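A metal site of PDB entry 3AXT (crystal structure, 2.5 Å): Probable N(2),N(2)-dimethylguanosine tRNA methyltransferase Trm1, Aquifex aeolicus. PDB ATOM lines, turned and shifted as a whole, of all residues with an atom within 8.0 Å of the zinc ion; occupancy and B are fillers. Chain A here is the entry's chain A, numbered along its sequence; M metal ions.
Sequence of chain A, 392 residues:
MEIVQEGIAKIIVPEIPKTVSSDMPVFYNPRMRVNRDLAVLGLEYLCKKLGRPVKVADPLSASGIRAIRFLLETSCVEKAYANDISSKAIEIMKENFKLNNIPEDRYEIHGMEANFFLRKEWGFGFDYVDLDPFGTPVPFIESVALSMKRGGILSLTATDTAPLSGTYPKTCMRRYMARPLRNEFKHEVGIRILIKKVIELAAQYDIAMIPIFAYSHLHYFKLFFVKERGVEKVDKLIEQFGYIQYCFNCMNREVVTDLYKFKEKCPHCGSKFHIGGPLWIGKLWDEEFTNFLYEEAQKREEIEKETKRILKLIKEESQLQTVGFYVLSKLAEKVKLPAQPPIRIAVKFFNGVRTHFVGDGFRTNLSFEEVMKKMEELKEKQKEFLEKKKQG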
ATOM      1  N   TYR A 246     -33.056  16.929   6.182  1.00  0.00           N
ATOM      2  CA  TYR A 246     -32.424  16.613   4.910  1.00  0.00           C
ATOM      3  C   TYR A 246     -32.357  17.820   3.982  1.00  0.00           C
ATOM      4  O   TYR A 246     -33.259  18.653   3.952  1.00  0.00           O
ATOM      5  CB  TYR A 246     -33.164  15.460   4.216  1.00  0.00           C
ATOM      6  CG  TYR A 246     -32.638  15.138   2.836  1.00  0.00           C
ATOM      7  CD1 TYR A 246     -33.246  15.656   1.703  1.00  0.00           C
ATOM      8  CD2 TYR A 246     -31.518  14.338   2.682  1.00  0.00           C
ATOM      9  CE1 TYR A 246     -32.756  15.366   0.444  1.00  0.00           C
ATOM     10  CE2 TYR A 246     -31.029  14.034   1.426  1.00  0.00           C
ATOM     11  CZ  TYR A 246     -31.649  14.562   0.309  1.00  0.00           C
ATOM     12  OH  TYR A 246     -31.166  14.265  -0.951  1.00  0.00           O
ATOM     13  N   CYS A 247     -31.253  17.905   3.237  1.00  0.00           N
ATOM     14  CA  CYS A 247     -31.042  19.001   2.303  1.00  0.00           C
ATOM     15  C   CYS A 247     -31.070  18.480   0.870  1.00  0.00           C
ATOM     16  O   CYS A 247     -30.267  17.632   0.491  1.00  0.00           O
ATOM     17  CB  CYS A 247     -29.711  19.679   2.597  1.00  0.00           C
ATOM     18  SG  CYS A 247     -29.299  21.032   1.482  1.00  0.00           S
ATOM     19  N   PHE A 248     -32.004  18.995   0.068  1.00  0.00           N
ATOM     20  CA  PHE A 248     -32.174  18.526  -1.295  1.00  0.00           C
ATOM     21  C   PHE A 248     -31.086  19.010  -2.249  1.00  0.00           C
ATOM     22  O   PHE A 248     -30.905  18.441  -3.328  1.00  0.00           O
ATOM     23  CB  PHE A 248     -33.551  18.917  -1.835  1.00  0.00           C
ATOM     24  CG  PHE A 248     -34.661  18.027  -1.371  1.00  0.00           C
ATOM     25  CD1 PHE A 248     -35.008  16.899  -2.100  1.00  0.00           C
ATOM     26  CD2 PHE A 248     -35.362  18.302  -0.202  1.00  0.00           C
ATOM     27  CE1 PHE A 248     -36.031  16.064  -1.678  1.00  0.00           C
ATOM     28  CE2 PHE A 248     -36.377  17.474   0.220  1.00  0.00           C
ATOM     29  CZ  PHE A 248     -36.715  16.351  -0.518  1.00  0.00           C
ATOM     30  N   ASN A 249     -30.359  20.046  -1.850  1.00  0.00           N
ATOM     31  CA  ASN A 249     -29.333  20.615  -2.710  1.00  0.00           C
ATOM     32  C   ASN A 249     -28.049  19.804  -2.728  1.00  0.00           C
ATOM     33  O   ASN A 249     -27.510  19.501  -3.794  1.00  0.00           O
ATOM     34  CB  ASN A 249     -29.042  22.060  -2.310  1.00  0.00           C
ATOM     35  CG  ASN A 249     -28.313  22.826  -3.387  1.00  0.00           C
ATOM     36  OD1 ASN A 249     -28.578  22.637  -4.578  1.00  0.00           O
ATOM     37  ND2 ASN A 249     -27.384  23.681  -2.986  1.00  0.00           N
ATOM     38  N   CYS A 250     -27.547  19.457  -1.540  1.00  0.00           N
ATOM     39  CA  CYS A 250     -26.277  18.751  -1.424  1.00  0.00           C
ATOM     40  C   CYS A 250     -26.439  17.381  -0.780  1.00  0.00           C
ATOM     41  O   CYS A 250     -25.467  16.644  -0.626  1.00  0.00           O
ATOM     42  CB  CYS A 250     -25.272  19.588  -0.634  1.00  0.00           C
ATOM     43  SG  CYS A 250     -25.704  19.750   1.105  1.00  0.00           S
ATOM     44  N   MET A 251     -27.669  17.055  -0.385  1.00  0.00           N
ATOM     45  CA  MET A 251     -27.995  15.736   0.146  1.00  0.00           C
ATOM     46  C   MET A 251     -27.527  15.511   1.584  1.00  0.00           C
ATOM     47  O   MET A 251     -27.468  14.378   2.056  1.00  0.00           O
ATOM     48  CB  MET A 251     -27.451  14.629  -0.758  1.00  0.00           C
ATOM     49  CG  MET A 251     -28.059  14.627  -2.154  1.00  0.00           C
ATOM     50  SD  MET A 251     -27.216  13.488  -3.272  1.00  0.00           S
ATOM     51  CE  MET A 251     -25.592  14.244  -3.364  1.00  0.00           C
ATOM     52  N   ASN A 252     -27.201  16.590   2.286  1.00  0.00           N
ATOM     53  CA  ASN A 252     -26.801  16.487   3.683  1.00  0.00           C
ATOM     54  C   ASN A 252     -27.975  16.062   4.563  1.00  0.00           C
ATOM     55  O   ASN A 252     -29.117  16.466   4.319  1.00  0.00           O
ATOM     56  CB  ASN A 252     -26.225  17.806   4.188  1.00  0.00           C
ATOM     57  CG  ASN A 252     -25.708  17.714   5.612  1.00  0.00           C
ATOM     58  OD1 ASN A 252     -25.315  16.649   6.078  1.00  0.00           O
ATOM     59  ND2 ASN A 252     -25.702  18.854   6.308  1.00  0.00           N
ATOM     60  N   ARG A 253     -27.699  15.257   5.578  1.00  0.00           N
ATOM     61  CA  ARG A 253     -28.757  14.774   6.465  1.00  0.00           C
ATOM     62  C   ARG A 253     -28.277  14.607   7.905  1.00  0.00           C
ATOM     63  O   ARG A 253     -27.107  14.327   8.163  1.00  0.00           O
ATOM     64  CB  ARG A 253     -29.353  13.462   5.954  1.00  0.00           C
ATOM     65  CG  ARG A 253     -28.488  12.225   6.203  1.00  0.00           C
ATOM     66  CD  ARG A 253     -27.205  12.266   5.385  1.00  0.00           C
ATOM     67  NE  ARG A 253     -27.461  12.396   3.955  1.00  0.00           N
ATOM     68  CZ  ARG A 253     -27.712  11.388   3.141  1.00  0.00           C
ATOM     69  NH1 ARG A 253     -27.940  11.612   1.856  1.00  0.00           N
ATOM     70  NH2 ARG A 253     -27.734  10.139   3.606  1.00  0.00           N
ATOM     71  N   LYS A 265     -31.276  26.287   8.189  1.00  0.00           N
ATOM     72  CA  LYS A 265     -30.382  26.243   7.031  1.00  0.00           C
ATOM     73  C   LYS A 265     -29.408  25.075   7.084  1.00  0.00           C
ATOM     74  O   LYS A 265     -28.866  24.736   8.133  1.00  0.00           O
ATOM     75  CB  LYS A 265     -29.627  27.564   6.898  1.00  0.00           C
ATOM     76  CG  LYS A 265     -30.510  28.752   6.550  1.00  0.00           C
ATOM     77  CD  LYS A 265     -31.340  28.457   5.306  1.00  0.00           C
ATOM     78  CE  LYS A 265     -32.253  29.618   4.966  1.00  0.00           C
ATOM     79  NZ  LYS A 265     -33.113  29.309   3.791  1.00  0.00           N
ATOM     80  N   CYS A 266     -29.190  24.460   5.918  1.00  0.00           N
ATOM     81  CA  CYS A 266     -28.239  23.377   5.779  1.00  0.00           C
ATOM     82  C   CYS A 266     -26.827  23.879   6.065  1.00  0.00           C
ATOM     83  O   CYS A 266     -26.326  24.768   5.379  1.00  0.00           O
ATOM     84  CB  CYS A 266     -28.323  22.783   4.378  1.00  0.00           C
ATOM     85  SG  CYS A 266     -26.944  21.714   3.933  1.00  0.00           S
ATOM     86  N   PRO A 267     -26.166  23.300   7.076  1.00  0.00           N
ATOM     87  CA  PRO A 267     -24.831  23.718   7.516  1.00  0.00           C
ATOM     88  C   PRO A 267     -23.786  23.665   6.397  1.00  0.00           C
ATOM     89  O   PRO A 267     -22.759  24.338   6.502  1.00  0.00           O
ATOM     90  CB  PRO A 267     -24.491  22.696   8.601  1.00  0.00           C
ATOM     91  CG  PRO A 267     -25.806  22.225   9.098  1.00  0.00           C
ATOM     92  CD  PRO A 267     -26.690  22.192   7.894  1.00  0.00           C
ATOM     93  N   HIS A 268     -24.044  22.879   5.360  1.00  0.00           N
ATOM     94  CA  HIS A 268     -23.072  22.700   4.290  1.00  0.00           C
ATOM     95  C   HIS A 268     -23.145  23.784   3.206  1.00  0.00           C
ATOM     96  O   HIS A 268     -22.155  24.464   2.944  1.00  0.00           O
ATOM     97  CB  HIS A 268     -23.234  21.320   3.646  1.00  0.00           C
ATOM     98  CG  HIS A 268     -22.195  21.005   2.620  1.00  0.00           C
ATOM     99  ND1 HIS A 268     -20.894  20.695   2.947  1.00  0.00           N
ATOM    100  CD2 HIS A 268     -22.265  20.939   1.264  1.00  0.00           C
ATOM    101  CE1 HIS A 268     -20.205  20.470   1.849  1.00  0.00           C
ATOM    102  NE2 HIS A 268     -21.013  20.607   0.818  1.00  0.00           N
ATOM    103  N   CYS A 269     -24.306  23.928   2.590  1.00  0.00           N
ATOM    104  CA  CYS A 269     -24.451  24.860   1.466  1.00  0.00           C
ATOM    105  C   CYS A 269     -25.446  25.981   1.754  1.00  0.00           C
ATOM    106  O   CYS A 269     -25.559  26.925   0.981  1.00  0.00           O
ATOM    107  CB  CYS A 269     -24.852  24.109   0.198  1.00  0.00           C
ATOM    108  SG  CYS A 269     -26.424  23.246   0.334  1.00  0.00           S
ATOM    109  N   GLY A 270     -26.164  25.871   2.870  1.00  0.00           N
ATOM    110  CA  GLY A 270     -27.030  26.943   3.325  1.00  0.00           C
ATOM    111  C   GLY A 270     -28.441  26.909   2.778  1.00  0.00           C
ATOM    112  O   GLY A 270     -29.245  27.803   3.064  1.00  0.00           O
ATOM    113  N   SER A 271     -28.759  25.880   2.005  1.00  0.00           N
ATOM    114  CA  SER A 271     -30.105  25.727   1.446  1.00  0.00           C
ATOM    115  C   SER A 271     -31.083  25.312   2.539  1.00  0.00           C
ATOM    116  O   SER A 271     -30.680  25.049   3.675  1.00  0.00           O
ATOM    117  CB  SER A 271     -30.107  24.697   0.320  1.00  0.00           C
ATOM    118  OG  SER A 271     -29.360  25.169  -0.788  1.00  0.00           O
ATOM    119  N   LYS A 272     -32.366  25.259   2.195  1.00  0.00           N
ATOM    120  CA  LYS A 272     -33.398  24.900   3.169  1.00  0.00           C
ATOM    121  C   LYS A 272     -33.199  23.491   3.709  1.00  0.00           C
ATOM    122  O   LYS A 272     -33.058  22.532   2.950  1.00  0.00           O
ATOM    123  CB  LYS A 272     -34.784  25.039   2.552  1.00  0.00           C
ATOM    124  CG  LYS A 272     -35.912  24.677   3.503  1.00  0.00           C
ATOM    125  CD  LYS A 272     -37.271  24.957   2.906  1.00  0.00           C
ATOM    126  CE  LYS A 272     -38.388  24.543   3.849  1.00  0.00           C
ATOM    127  NZ  LYS A 272     -38.301  25.247   5.155  1.00  0.00           N
ATOM    128  N   PHE A 273     -33.196  23.371   5.034  1.00  0.00           N
ATOM    129  CA  PHE A 273     -33.031  22.088   5.699  1.00  0.00           C
ATOM    130  C   PHE A 273     -34.388  21.508   6.082  1.00  0.00           C
ATOM    131  O   PHE A 273     -34.920  21.805   7.151  1.00  0.00           O
ATOM    132  CB  PHE A 273     -32.171  22.241   6.958  1.00  0.00           C
ATOM    133  CG  PHE A 273     -31.234  21.102   7.194  1.00  0.00           C
ATOM    134  CD1 PHE A 273     -31.076  20.106   6.247  1.00  0.00           C
ATOM    135  CD2 PHE A 273     -30.507  21.010   8.375  1.00  0.00           C
ATOM    136  CE1 PHE A 273     -30.212  19.052   6.470  1.00  0.00           C
ATOM    137  CE2 PHE A 273     -29.642  19.956   8.598  1.00  0.00           C
ATOM    138  CZ  PHE A 273     -29.491  18.980   7.645  1.00  0.00           C
ATOM    139  N   LYS A 334     -22.822  15.038  -8.343  1.00  0.00           N
ATOM    140  CA  LYS A 334     -22.584  16.271  -7.598  1.00  0.00           C
ATOM    141  C   LYS A 334     -21.149  16.753  -7.744  1.00  0.00           C
ATOM    142  O   LYS A 334     -20.893  17.956  -7.807  1.00  0.00           O
ATOM    143  CB  LYS A 334     -22.912  16.063  -6.116  1.00  0.00           C
ATOM    144  CG  LYS A 334     -22.968  17.342  -5.306  1.00  0.00           C
ATOM    145  CD  LYS A 334     -24.222  18.150  -5.627  1.00  0.00           C
ATOM    146  CE  LYS A 334     -24.231  19.483  -4.900  1.00  0.00           C
ATOM    147  NZ  LYS A 334     -23.129  20.369  -5.354  1.00  0.00           N
ATOM    148  N   PHE A 368     -21.353  13.189   6.814  1.00  0.00           N
ATOM    149  CA  PHE A 368     -21.611  13.737   5.488  1.00  0.00           C
ATOM    150  C   PHE A 368     -20.376  14.441   4.924  1.00  0.00           C
ATOM    151  O   PHE A 368     -20.028  14.270   3.754  1.00  0.00           O
ATOM    152  CB  PHE A 368     -22.799  14.692   5.511  1.00  0.00           C
ATOM    153  CG  PHE A 368     -23.073  15.365   4.198  1.00  0.00           C
ATOM    154  CD1 PHE A 368     -22.682  16.680   3.977  1.00  0.00           C
ATOM    155  CD2 PHE A 368     -23.708  14.680   3.174  1.00  0.00           C
ATOM    156  CE1 PHE A 368     -22.926  17.294   2.767  1.00  0.00           C
ATOM    157  CE2 PHE A 368     -23.952  15.294   1.964  1.00  0.00           C
ATOM    158  CZ  PHE A 368     -23.564  16.596   1.755  1.00  0.00           C
HETATM  159 ZN    ZN M   1     -27.063  21.493   1.641  1.00  0.00          ZN
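Within 4 Å of the zinc ion: Cys 247, Cys 250, Cys 266 and Cys 269.
The zinc ion is bound by the side-chain sulfur of Cys 250 (2.3 Å), the side-chain sulfur of Cys 269 (2.3 Å), the side-chain sulfur of Cys 247 (2.3 Å) and the side-chain sulfur of Cys 266 (2.3 Å).
The zinc ion has four donor atoms within binding distance.
The backbone NH (N) of Asn 252 sits close to the side-chain sulfur (SG) of Cys 250 (3.7 Å).
SG of Cys 269 sits close to ND2 of Asn 249 (3.5 Å).
The side-chain sulfur (SG) of Cys 269 sits close to the side-chain hydroxyl (OG) of Ser 271, at 3.7 Å.
SG of Cys 247 sits close to N of Asn 249 (3.6 Å).
The backbone carbonyl oxygen (O) of Asn 252 is in hydrogen-bond range of the backbone NH (N) of Cys 247, at 2.8 Å.
SG of Cys 266 lies close to N of His 268, at 3.4 Å.
The backbone NH (N) of Cys 266 is in hydrogen-bond range of the backbone carbonyl oxygen (O) of Ser 271.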
